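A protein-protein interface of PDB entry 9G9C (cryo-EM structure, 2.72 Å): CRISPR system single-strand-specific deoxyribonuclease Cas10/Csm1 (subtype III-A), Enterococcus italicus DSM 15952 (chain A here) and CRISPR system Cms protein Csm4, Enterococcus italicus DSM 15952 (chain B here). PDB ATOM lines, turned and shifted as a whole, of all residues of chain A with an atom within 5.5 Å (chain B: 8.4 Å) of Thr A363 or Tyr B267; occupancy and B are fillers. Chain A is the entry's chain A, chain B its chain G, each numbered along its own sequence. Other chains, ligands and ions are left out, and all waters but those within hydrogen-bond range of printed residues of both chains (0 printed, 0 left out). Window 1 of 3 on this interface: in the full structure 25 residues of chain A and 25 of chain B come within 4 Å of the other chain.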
ATOM      1  N   PHE A 357      17.016  -5.638 -40.254  1.00  0.00           N
ATOM      2  CA  PHE A 357      16.077  -5.880 -39.166  1.00  0.00           C
ATOM      3  C   PHE A 357      15.683  -4.582 -38.478  1.00  0.00           C
ATOM      4  O   PHE A 357      14.530  -4.424 -38.064  1.00  0.00           O
ATOM      5  CB  PHE A 357      16.667  -6.877 -38.169  1.00  0.00           C
ATOM      6  CG  PHE A 357      16.424  -8.311 -38.541  1.00  0.00           C
ATOM      7  CD1 PHE A 357      15.241  -8.937 -38.190  1.00  0.00           C
ATOM      8  CD2 PHE A 357      17.366  -9.026 -39.257  1.00  0.00           C
ATOM      9  CE1 PHE A 357      15.010 -10.253 -38.533  1.00  0.00           C
ATOM     10  CE2 PHE A 357      17.138 -10.340 -39.607  1.00  0.00           C
ATOM     11  CZ  PHE A 357      15.961 -10.955 -39.243  1.00  0.00           C
ATOM     12  N   PHE A 361      11.735  -4.311 -38.760  1.00  0.00           N
ATOM     13  CA  PHE A 361      10.991  -4.588 -37.502  1.00  0.00           C
ATOM     14  C   PHE A 361      11.485  -3.719 -36.363  1.00  0.00           C
ATOM     15  O   PHE A 361      10.942  -3.869 -35.249  1.00  0.00           O
ATOM     16  CB  PHE A 361      11.139  -6.054 -37.085  1.00  0.00           C
ATOM     17  CG  PHE A 361      10.850  -7.093 -38.158  1.00  0.00           C
ATOM     18  CD1 PHE A 361       9.550  -7.518 -38.405  1.00  0.00           C
ATOM     19  CD2 PHE A 361      11.881  -7.666 -38.890  1.00  0.00           C
ATOM     20  CE1 PHE A 361       9.289  -8.471 -39.375  1.00  0.00           C
ATOM     21  CE2 PHE A 361      11.614  -8.621 -39.856  1.00  0.00           C
ATOM     22  CZ  PHE A 361      10.322  -9.020 -40.097  1.00  0.00           C
ATOM     23  N   LYS A 362      12.487  -2.865 -36.593  1.00  0.00           N
ATOM     24  CA  LYS A 362      13.084  -2.048 -35.498  1.00  0.00           C
ATOM     25  C   LYS A 362      13.629  -2.985 -34.406  1.00  0.00           C
ATOM     26  O   LYS A 362      14.474  -3.836 -34.735  1.00  0.00           O
ATOM     27  CB  LYS A 362      12.086  -1.043 -34.912  1.00  0.00           C
ATOM     28  CG  LYS A 362      11.600   0.030 -35.868  1.00  0.00           C
ATOM     29  CD  LYS A 362      12.679   1.058 -36.181  1.00  0.00           C
ATOM     30  CE  LYS A 362      12.227   2.053 -37.198  1.00  0.00           C
ATOM     31  NZ  LYS A 362      11.009   2.740 -36.763  1.00  0.00           N
ATOM     32  N   THR A 363      13.167  -2.827 -33.163  1.00  0.00           N
ATOM     33  CA  THR A 363      13.653  -3.670 -32.050  1.00  0.00           C
ATOM     34  C   THR A 363      12.797  -4.916 -31.868  1.00  0.00           C
ATOM     35  O   THR A 363      13.041  -5.633 -30.876  1.00  0.00           O
ATOM     36  CB  THR A 363      13.694  -2.818 -30.783  1.00  0.00           C
ATOM     37  OG1 THR A 363      12.365  -2.336 -30.619  1.00  0.00           O
ATOM     38  CG2 THR A 363      14.658  -1.652 -30.898  1.00  0.00           C
ATOM     39  N   ASP A 364      11.836  -5.195 -32.755  1.00  0.00           N
ATOM     40  CA  ASP A 364      10.984  -6.359 -32.525  1.00  0.00           C
ATOM     41  C   ASP A 364      11.736  -7.659 -32.785  1.00  0.00           C
ATOM     42  O   ASP A 364      11.550  -8.644 -32.060  1.00  0.00           O
ATOM     43  CB  ASP A 364       9.733  -6.273 -33.399  1.00  0.00           C
ATOM     44  CG  ASP A 364       8.769  -5.197 -32.934  1.00  0.00           C
ATOM     45  OD1 ASP A 364       9.042  -4.558 -31.897  1.00  0.00           O
ATOM     46  OD2 ASP A 364       7.739  -4.987 -33.609  1.00  0.00           O
ATOM     47  N   LEU A 365      12.585  -7.684 -33.810  1.00  0.00           N
ATOM     48  CA  LEU A 365      13.384  -8.855 -34.141  1.00  0.00           C
ATOM     49  C   LEU A 365      14.827  -8.438 -34.374  1.00  0.00           C
ATOM     50  O   LEU A 365      15.101  -7.333 -34.851  1.00  0.00           O
ATOM     51  CB  LEU A 365      12.850  -9.575 -35.386  1.00  0.00           C
ATOM     52  CG  LEU A 365      11.504 -10.281 -35.260  1.00  0.00           C
ATOM     53  CD1 LEU A 365      11.015 -10.729 -36.621  1.00  0.00           C
ATOM     54  CD2 LEU A 365      11.630 -11.466 -34.328  1.00  0.00           C
ATOM     55  N   TYR A 405      22.607  -2.615 -30.082  1.00  0.00           N
ATOM     56  CA  TYR A 405      22.486  -1.498 -31.066  1.00  0.00           C
ATOM     57  C   TYR A 405      23.587  -0.447 -30.936  1.00  0.00           C
ATOM     58  O   TYR A 405      23.910  -0.016 -29.818  1.00  0.00           O
ATOM     59  CB  TYR A 405      21.097  -0.860 -30.964  1.00  0.00           C
ATOM     60  CG  TYR A 405      19.953  -1.848 -31.143  1.00  0.00           C
ATOM     61  CD1 TYR A 405      19.584  -2.286 -32.407  1.00  0.00           C
ATOM     62  CD2 TYR A 405      19.239  -2.327 -30.054  1.00  0.00           C
ATOM     63  CE1 TYR A 405      18.548  -3.187 -32.582  1.00  0.00           C
ATOM     64  CE2 TYR A 405      18.198  -3.225 -30.216  1.00  0.00           C
ATOM     65  CZ  TYR A 405      17.852  -3.656 -31.484  1.00  0.00           C
ATOM     66  OH  TYR A 405      16.832  -4.544 -31.653  1.00  0.00           O
ATOM     67  N   ILE A 410      20.678   3.731 -32.353  1.00  0.00           N
ATOM     68  CA  ILE A 410      19.884   4.130 -31.151  1.00  0.00           C
ATOM     69  C   ILE A 410      19.372   5.563 -31.349  1.00  0.00           C
ATOM     70  O   ILE A 410      18.179   5.812 -31.078  1.00  0.00           O
ATOM     71  CB  ILE A 410      20.730   4.001 -29.871  1.00  0.00           C
ATOM     72  CG1 ILE A 410      21.134   2.555 -29.621  1.00  0.00           C
ATOM     73  CG2 ILE A 410      20.005   4.591 -28.663  1.00  0.00           C
ATOM     74  CD1 ILE A 410      21.692   2.299 -28.235  1.00  0.00           C
ATOM     75  N   PHE A 413      16.472   5.507 -33.855  1.00  0.00           N
ATOM     76  CA  PHE A 413      15.193   5.051 -33.263  1.00  0.00           C
ATOM     77  C   PHE A 413      14.583   6.196 -32.498  1.00  0.00           C
ATOM     78  O   PHE A 413      13.364   6.435 -32.613  1.00  0.00           O
ATOM     79  CB  PHE A 413      15.551   4.003 -32.212  1.00  0.00           C
ATOM     80  CG  PHE A 413      15.974   2.616 -32.671  1.00  0.00           C
ATOM     81  CD1 PHE A 413      15.414   2.025 -33.797  1.00  0.00           C
ATOM     82  CD2 PHE A 413      16.926   1.900 -31.955  1.00  0.00           C
ATOM     83  CE1 PHE A 413      15.804   0.756 -34.192  1.00  0.00           C
ATOM     84  CE2 PHE A 413      17.316   0.636 -32.360  1.00  0.00           C
ATOM     85  CZ  PHE A 413      16.753   0.067 -33.476  1.00  0.00           C
ATOM     86  N   ASN A 414      15.414   6.912 -31.743  1.00  0.00           N
ATOM     87  CA  ASN A 414      14.962   8.086 -30.944  1.00  0.00           C
ATOM     88  C   ASN A 414      14.466   9.225 -31.841  1.00  0.00           C
ATOM     89  O   ASN A 414      13.496   9.898 -31.436  1.00  0.00           O
ATOM     90  CB  ASN A 414      16.007   8.507 -29.915  1.00  0.00           C
ATOM     91  CG  ASN A 414      16.095   7.509 -28.788  1.00  0.00           C
ATOM     92  OD1 ASN A 414      15.078   7.187 -28.167  1.00  0.00           O
ATOM     93  ND2 ASN A 414      17.286   6.991 -28.526  1.00  0.00           N
ATOM     94  N   ASP B  34       9.152   7.137 -15.965  1.00  0.00           N
ATOM     95  CA  ASP B  34       8.474   8.121 -16.850  1.00  0.00           C
ATOM     96  C   ASP B  34       6.970   8.092 -16.579  1.00  0.00           C
ATOM     97  O   ASP B  34       6.365   9.177 -16.502  1.00  0.00           O
ATOM     98  CB  ASP B  34       8.831   7.873 -18.307  1.00  0.00           C
ATOM     99  CG  ASP B  34       8.769   6.426 -18.775  1.00  0.00           C
ATOM    100  OD1 ASP B  34       7.669   5.840 -18.732  1.00  0.00           O
ATOM    101  OD2 ASP B  34       9.823   5.902 -19.191  1.00  0.00           O
ATOM    102  N   SER B 225      14.422   3.763 -15.976  1.00  0.00           N
ATOM    103  CA  SER B 225      14.469   3.615 -17.454  1.00  0.00           C
ATOM    104  C   SER B 225      14.972   4.953 -18.001  1.00  0.00           C
ATOM    105  O   SER B 225      14.202   5.931 -17.937  1.00  0.00           O
ATOM    106  CB  SER B 225      13.126   3.262 -18.015  1.00  0.00           C
ATOM    107  OG  SER B 225      13.215   2.974 -19.403  1.00  0.00           O
ATOM    108  N   ALA B 226      16.201   5.002 -18.518  1.00  0.00           N
ATOM    109  CA  ALA B 226      16.792   6.308 -18.896  1.00  0.00           C
ATOM    110  C   ALA B 226      17.468   6.287 -20.265  1.00  0.00           C
ATOM    111  O   ALA B 226      17.866   5.203 -20.721  1.00  0.00           O
ATOM    112  CB  ALA B 226      17.787   6.696 -17.839  1.00  0.00           C
ATOM    113  N   MET B 227      17.587   7.464 -20.883  1.00  0.00           N
ATOM    114  CA  MET B 227      18.276   7.590 -22.192  1.00  0.00           C
ATOM    115  C   MET B 227      19.222   8.795 -22.123  1.00  0.00           C
ATOM    116  O   MET B 227      18.834   9.823 -21.533  1.00  0.00           O
ATOM    117  CB  MET B 227      17.278   7.756 -23.343  1.00  0.00           C
ATOM    118  CG  MET B 227      17.909   8.029 -24.695  1.00  0.00           C
ATOM    119  SD  MET B 227      19.264   6.914 -25.111  1.00  0.00           S
ATOM    120  CE  MET B 227      18.417   5.331 -25.176  1.00  0.00           C
ATOM    121  N   ALA B 228      20.415   8.664 -22.700  1.00  0.00           N
ATOM    122  CA  ALA B 228      21.432   9.738 -22.657  1.00  0.00           C
ATOM    123  C   ALA B 228      21.219  10.765 -23.762  1.00  0.00           C
ATOM    124  O   ALA B 228      20.533  10.464 -24.760  1.00  0.00           O
ATOM    125  CB  ALA B 228      22.794   9.115 -22.809  1.00  0.00           C
ATOM    126  N   LEU B 233      25.550   9.957 -25.293  1.00  0.00           N
ATOM    127  CA  LEU B 233      25.401   8.580 -25.836  1.00  0.00           C
ATOM    128  C   LEU B 233      26.730   8.062 -26.392  1.00  0.00           C
ATOM    129  O   LEU B 233      27.033   6.873 -26.167  1.00  0.00           O
ATOM    130  CB  LEU B 233      24.316   8.543 -26.913  1.00  0.00           C
ATOM    131  CG  LEU B 233      23.765   7.161 -27.269  1.00  0.00           C
ATOM    132  CD1 LEU B 233      23.101   6.551 -26.055  1.00  0.00           C
ATOM    133  CD2 LEU B 233      22.769   7.268 -28.405  1.00  0.00           C
ATOM    134  N   LEU B 243      19.435  -2.930 -22.385  1.00  0.00           N
ATOM    135  CA  LEU B 243      18.262  -3.500 -23.046  1.00  0.00           C
ATOM    136  C   LEU B 243      17.372  -2.332 -23.460  1.00  0.00           C
ATOM    137  O   LEU B 243      16.702  -1.732 -22.615  1.00  0.00           O
ATOM    138  CB  LEU B 243      17.531  -4.475 -22.132  1.00  0.00           C
ATOM    139  CG  LEU B 243      16.432  -5.365 -22.727  1.00  0.00           C
ATOM    140  CD1 LEU B 243      15.070  -4.686 -22.707  1.00  0.00           C
ATOM    141  CD2 LEU B 243      16.794  -5.795 -24.141  1.00  0.00           C
ATOM    142  N   LEU B 244      17.481  -1.921 -24.725  1.00  0.00           N
ATOM    143  CA  LEU B 244      16.669  -0.788 -25.241  1.00  0.00           C
ATOM    144  C   LEU B 244      15.189  -1.163 -25.121  1.00  0.00           C
ATOM    145  O   LEU B 244      14.770  -2.142 -25.769  1.00  0.00           O
ATOM    146  CB  LEU B 244      17.027  -0.453 -26.687  1.00  0.00           C
ATOM    147  CG  LEU B 244      17.925   0.768 -26.896  1.00  0.00           C
ATOM    148  CD1 LEU B 244      18.020   1.067 -28.378  1.00  0.00           C
ATOM    149  CD2 LEU B 244      17.348   1.954 -26.154  1.00  0.00           C
ATOM    150  N   LYS B 245      14.438  -0.403 -24.327  1.00  0.00           N
ATOM    151  CA  LYS B 245      12.992  -0.678 -24.179  1.00  0.00           C
ATOM    152  C   LYS B 245      12.250   0.417 -24.938  1.00  0.00           C
ATOM    153  O   LYS B 245      12.509   1.607 -24.668  1.00  0.00           O
ATOM    154  CB  LYS B 245      12.599  -0.629 -22.703  1.00  0.00           C
ATOM    155  CG  LYS B 245      11.145  -0.943 -22.395  1.00  0.00           C
ATOM    156  CD  LYS B 245      10.678  -0.261 -21.116  1.00  0.00           C
ATOM    157  CE  LYS B 245      11.726  -0.260 -20.051  1.00  0.00           C
ATOM    158  NZ  LYS B 245      11.257   0.415 -18.839  1.00  0.00           N
ATOM    159  N   LYS B 246      11.377   0.022 -25.860  1.00  0.00           N
ATOM    160  CA  LYS B 246      10.569   1.040 -26.563  1.00  0.00           C
ATOM    161  C   LYS B 246       9.656   1.702 -25.535  1.00  0.00           C
ATOM    162  O   LYS B 246       9.038   0.971 -24.735  1.00  0.00           O
ATOM    163  CB  LYS B 246       9.731   0.347 -27.640  1.00  0.00           C
ATOM    164  CG  LYS B 246       9.019   1.229 -28.650  1.00  0.00           C
ATOM    165  CD  LYS B 246       8.436   0.361 -29.760  1.00  0.00           C
ATOM    166  CE  LYS B 246       7.706   1.122 -30.818  1.00  0.00           C
ATOM    167  NZ  LYS B 246       8.552   2.146 -31.434  1.00  0.00           N
ATOM    168  N   ARG B 247       9.568   3.031 -25.551  1.00  0.00           N
ATOM    169  CA  ARG B 247       8.650   3.764 -24.649  1.00  0.00           C
ATOM    170  C   ARG B 247       7.608   4.447 -25.540  1.00  0.00           C
ATOM    171  O   ARG B 247       7.950   5.477 -26.150  1.00  0.00           O
ATOM    172  CB  ARG B 247       9.463   4.772 -23.835  1.00  0.00           C
ATOM    173  CG  ARG B 247      10.691   4.227 -23.123  1.00  0.00           C
ATOM    174  CD  ARG B 247      10.334   3.173 -22.091  1.00  0.00           C
ATOM    175  NE  ARG B 247       9.315   3.631 -21.140  1.00  0.00           N
ATOM    176  CZ  ARG B 247       8.137   3.046 -20.970  1.00  0.00           C
ATOM    177  NH1 ARG B 247       7.860   1.922 -21.606  1.00  0.00           N
ATOM    178  NH2 ARG B 247       7.238   3.586 -20.171  1.00  0.00           N
ATOM    179  N   THR B 248       6.396   3.901 -25.622  1.00  0.00           N
ATOM    180  CA  THR B 248       5.378   4.440 -26.557  1.00  0.00           C
ATOM    181  C   THR B 248       4.043   4.586 -25.864  1.00  0.00           C
ATOM    182  O   THR B 248       3.864   3.951 -24.809  1.00  0.00           O
ATOM    183  CB  THR B 248       5.260   3.524 -27.774  1.00  0.00           C
ATOM    184  OG1 THR B 248       5.181   2.199 -27.262  1.00  0.00           O
ATOM    185  CG2 THR B 248       6.449   3.649 -28.706  1.00  0.00           C
ATOM    186  N   LYS B 264       5.395  10.662 -29.761  1.00  0.00           N
ATOM    187  CA  LYS B 264       6.490  10.175 -30.638  1.00  0.00           C
ATOM    188  C   LYS B 264       7.140   8.959 -29.958  1.00  0.00           C
ATOM    189  O   LYS B 264       7.319   8.995 -28.722  1.00  0.00           O
ATOM    190  CB  LYS B 264       7.494  11.294 -30.927  1.00  0.00           C
ATOM    191  CG  LYS B 264       6.963  12.396 -31.830  1.00  0.00           C
ATOM    192  CD  LYS B 264       8.084  13.297 -32.325  1.00  0.00           C
ATOM    193  CE  LYS B 264       8.980  13.695 -31.199  1.00  0.00           C
ATOM    194  NZ  LYS B 264      10.130  14.466 -31.672  1.00  0.00           N
ATOM    195  N   ASP B 265       7.485   7.926 -30.734  1.00  0.00           N
ATOM    196  CA  ASP B 265       8.084   6.684 -30.171  1.00  0.00           C
ATOM    197  C   ASP B 265       9.466   6.990 -29.594  1.00  0.00           C
ATOM    198  O   ASP B 265      10.252   7.680 -30.275  1.00  0.00           O
ATOM    199  CB  ASP B 265       8.159   5.588 -31.219  1.00  0.00           C
ATOM    200  CG  ASP B 265       6.846   5.239 -31.905  1.00  0.00           C
ATOM    201  OD1 ASP B 265       5.830   5.895 -31.595  1.00  0.00           O
ATOM    202  OD2 ASP B 265       6.851   4.306 -32.734  1.00  0.00           O
ATOM    203  N   PHE B 266       9.752   6.484 -28.394  1.00  0.00           N
ATOM    204  CA  PHE B 266      11.051   6.757 -27.732  1.00  0.00           C
ATOM    205  C   PHE B 266      11.643   5.435 -27.296  1.00  0.00           C
ATOM    206  O   PHE B 266      10.883   4.515 -26.981  1.00  0.00           O
ATOM    207  CB  PHE B 266      10.816   7.723 -26.570  1.00  0.00           C
ATOM    208  CG  PHE B 266      12.075   8.143 -25.826  1.00  0.00           C
ATOM    209  CD1 PHE B 266      12.881   9.159 -26.319  1.00  0.00           C
ATOM    210  CD2 PHE B 266      12.430   7.539 -24.627  1.00  0.00           C
ATOM    211  CE1 PHE B 266      14.025   9.542 -25.643  1.00  0.00           C
ATOM    212  CE2 PHE B 266      13.572   7.932 -23.952  1.00  0.00           C
ATOM    213  CZ  PHE B 266      14.363   8.931 -24.461  1.00  0.00           C
ATOM    214  N   TYR B 267      12.969   5.347 -27.284  1.00  0.00           N
ATOM    215  CA  TYR B 267      13.651   4.101 -26.855  1.00  0.00           C
ATOM    216  C   TYR B 267      14.544   4.462 -25.698  1.00  0.00           C
ATOM    217  O   TYR B 267      15.321   5.417 -25.821  1.00  0.00           O
ATOM    218  CB  TYR B 267      14.391   3.525 -28.065  1.00  0.00           C
ATOM    219  CG  TYR B 267      13.483   2.951 -29.142  1.00  0.00           C
ATOM    220  CD1 TYR B 267      12.907   3.768 -30.106  1.00  0.00           C
ATOM    221  CD2 TYR B 267      13.215   1.591 -29.198  1.00  0.00           C
ATOM    222  CE1 TYR B 267      12.081   3.252 -31.089  1.00  0.00           C
ATOM    223  CE2 TYR B 267      12.394   1.062 -30.178  1.00  0.00           C
ATOM    224  CZ  TYR B 267      11.827   1.894 -31.126  1.00  0.00           C
ATOM    225  OH  TYR B 267      11.019   1.377 -32.094  1.00  0.00           O
ATOM    226  N   ALA B 268      14.418   3.739 -24.589  1.00  0.00           N
ATOM    227  CA  ALA B 268      15.199   4.079 -23.379  1.00  0.00           C
ATOM    228  C   ALA B 268      15.919   2.839 -22.859  1.00  0.00           C
ATOM    229  O   ALA B 268      15.350   1.735 -22.947  1.00  0.00           O
ATOM    230  CB  ALA B 268      14.283   4.652 -22.327  1.00  0.00           C
ATOM    231  N   PHE B 269      17.122   3.015 -22.314  1.00  0.00           N
ATOM    232  CA  PHE B 269      17.845   1.875 -21.693  1.00  0.00           C
ATOM    233  C   PHE B 269      17.039   1.430 -20.493  1.00  0.00           C
ATOM    234  O   PHE B 269      16.599   2.300 -19.722  1.00  0.00           O
ATOM    235  CB  PHE B 269      19.237   2.375 -21.318  1.00  0.00           C
ATOM    236  CG  PHE B 269      20.093   2.772 -22.510  1.00  0.00           C
ATOM    237  CD1 PHE B 269      20.153   1.969 -23.642  1.00  0.00           C
ATOM    238  CD2 PHE B 269      20.815   3.959 -22.503  1.00  0.00           C
ATOM    239  CE1 PHE B 269      20.936   2.331 -24.722  1.00  0.00           C
ATOM    240  CE2 PHE B 269      21.598   4.315 -23.587  1.00  0.00           C
ATOM    241  CZ  PHE B 269      21.652   3.503 -24.695  1.00  0.00           C
ATOM    242  N   SER B 270      16.868   0.123 -20.308  1.00  0.00           N
ATOM    243  CA  SER B 270      15.978  -0.372 -19.229  1.00  0.00           C
ATOM    244  C   SER B 270      16.668  -0.290 -17.867  1.00  0.00           C
ATOM    245  O   SER B 270      17.899  -0.107 -17.830  1.00  0.00           O
ATOM    246  CB  SER B 270      15.539  -1.779 -19.499  1.00  0.00           C
ATOM    247  OG  SER B 270      14.882  -1.871 -20.755  1.00  0.00           O
ATOM    248  N   PHE B 284      12.944  14.367 -22.184  1.00  0.00           N
ATOM    249  CA  PHE B 284      12.727  14.522 -23.614  1.00  0.00           C
ATOM    250  C   PHE B 284      11.296  14.975 -23.893  1.00  0.00           C
ATOM    251  O   PHE B 284      10.420  14.933 -23.029  1.00  0.00           O
ATOM    252  CB  PHE B 284      13.037  13.218 -24.349  1.00  0.00           C
ATOM    253  CG  PHE B 284      14.500  12.875 -24.383  1.00  0.00           C
ATOM    254  CD1 PHE B 284      15.081  12.159 -23.352  1.00  0.00           C
ATOM    255  CD2 PHE B 284      15.294  13.268 -25.445  1.00  0.00           C
ATOM    256  CE1 PHE B 284      16.423  11.841 -23.379  1.00  0.00           C
ATOM    257  CE2 PHE B 284      16.639  12.952 -25.478  1.00  0.00           C
ATOM    258  CZ  PHE B 284      17.203  12.238 -24.442  1.00  0.00           C
ATOM    259  N   VAL B 286       8.237  14.186 -26.342  1.00  0.00           N
ATOM    260  CA  VAL B 286       7.673  13.217 -27.323  1.00  0.00           C
ATOM    261  C   VAL B 286       6.395  13.800 -27.941  1.00  0.00           C
ATOM    262  O   VAL B 286       5.609  13.021 -28.511  1.00  0.00           O
ATOM    263  CB  VAL B 286       7.404  11.872 -26.624  1.00  0.00           C
ATOM    264  CG1 VAL B 286       8.697  11.118 -26.342  1.00  0.00           C
ATOM    265  CG2 VAL B 286       6.598  12.044 -25.344  1.00  0.00           C
ATOM    266  N   ARG B 296       8.741  13.362 -21.515  1.00  0.00           N
ATOM    267  CA  ARG B 296       9.008  11.931 -21.218  1.00  0.00           C
ATOM    268  C   ARG B 296      10.290  11.851 -20.377  1.00  0.00           C
ATOM    269  O   ARG B 296      11.382  12.134 -20.920  1.00  0.00           O
ATOM    270  CB  ARG B 296       9.133  11.078 -22.485  1.00  0.00           C
ATOM    271  CG  ARG B 296       9.374   9.616 -22.137  1.00  0.00           C
ATOM    272  CD  ARG B 296       9.373   8.701 -23.349  1.00  0.00           C
ATOM    273  NE  ARG B 296       8.051   8.336 -23.875  1.00  0.00           N
ATOM    274  CZ  ARG B 296       7.152   7.561 -23.274  1.00  0.00           C
ATOM    275  NH1 ARG B 296       7.393   7.051 -22.079  1.00  0.00           N
ATOM    276  NH2 ARG B 296       6.015   7.284 -23.886  1.00  0.00           N
ATOM    277  N   ALA B 298      13.548  10.652 -18.785  1.00  0.00           N
ATOM    278  CA  ALA B 298      14.560   9.683 -19.251  1.00  0.00           C
ATOM    279  C   ALA B 298      15.802  10.010 -18.438  1.00  0.00           C
ATOM    280  O   ALA B 298      16.915   9.609 -18.816  1.00  0.00           O
ATOM    281  CB  ALA B 298      14.792   9.823 -20.728  1.00  0.00           C
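Hydrophobic or aromatic side chains of chain B that line the printed part of chain A: Met B227, Leu B233, Leu B244, Phe B266, Tyr B267 and Phe B269. Among the printed residues, 12 pairs touch across the chains.
Lys A362 touches Tyr B267 (CB to OH, 3.9 Å). Thr A363 touches Tyr B267 (OG1 to CE2, 3.4 Å). Tyr A405 touches Leu B244 (CD2 to CD1, 3.98 Å). CD2 of Leu B233 touches CG2 of Ile A410, at 3.9 Å. Ile A410 touches Leu B244. CD1 of Ile A410 touches CE1 of Phe B269 (3.6 Å). Leu B244 touches Phe A413 (CD1 to CD2, 3.8 Å). Phe A413 touches Tyr B267 (CB to CD1, 3.4 Å). Asn A414 touches Met B227 (ND2 to CE, 3.9 Å). OD1 of Asn A414 touches CD1 of Phe B266 (3.5 Å).
Asp A364 touches none of the printed residues of chain B. Of the printed residues of chain B, Phe A413 touches Leu B244 and Tyr B267. Of the printed residues of chain A, Leu B244 touches Tyr A405 (3.98 Å), Ile A410 (3.7 Å) and Phe A413 (3.8 Å). Tyr B267 touches just these residues of chain A: Lys A362 (3.9 Å), Thr A363 (3.4 Å), Phe A413 (3.4 Å) and Asn A414 (2.9 Å). Of the printed residues of chain A, Phe B269 touches Ile A410 (3.6 Å). Phe B284 touches none of the printed residues of chain A. The nearest residue of chain B that does not touch Thr A363 is Lys B246 (4.8 Å). The nearest residue of chain A that does not touch Tyr B267 is Ile A410 (5.4 Å). The nearest printed residue of chain A that does not touch Phe B269 is Tyr A405 (6.3 Å).
The side-chain amide oxygen of Asn A414 sits at hydrogen-bond distance from the backbone NH of Tyr B267, 2.9 Å away.
ND2 of Asn A414 lies within hydrogen-bond range of O of Ile A410 (2.9 Å). The side-chain amino group of Lys B246 is in hydrogen-bond range of the side-chain hydroxyl of Tyr B267 (2.7 Å). The backbone carbonyl oxygen (O) of Phe A357 is in hydrogen-bond range of the backbone NH (N) of Lys A362 (3.0 Å). The backbone carbonyl oxygen (O) of Ala B298 is in hydrogen-bond range of the backbone NH (N) of Met B227. The backbone NH (N) of Arg B247 sits at hydrogen-bond distance from the backbone carbonyl oxygen (O) of Phe B266 (2.4 Å). The backbone NH (N) of Phe B269 is in hydrogen-bond range of the backbone carbonyl oxygen (O) of Ala B226 (2.8 Å).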
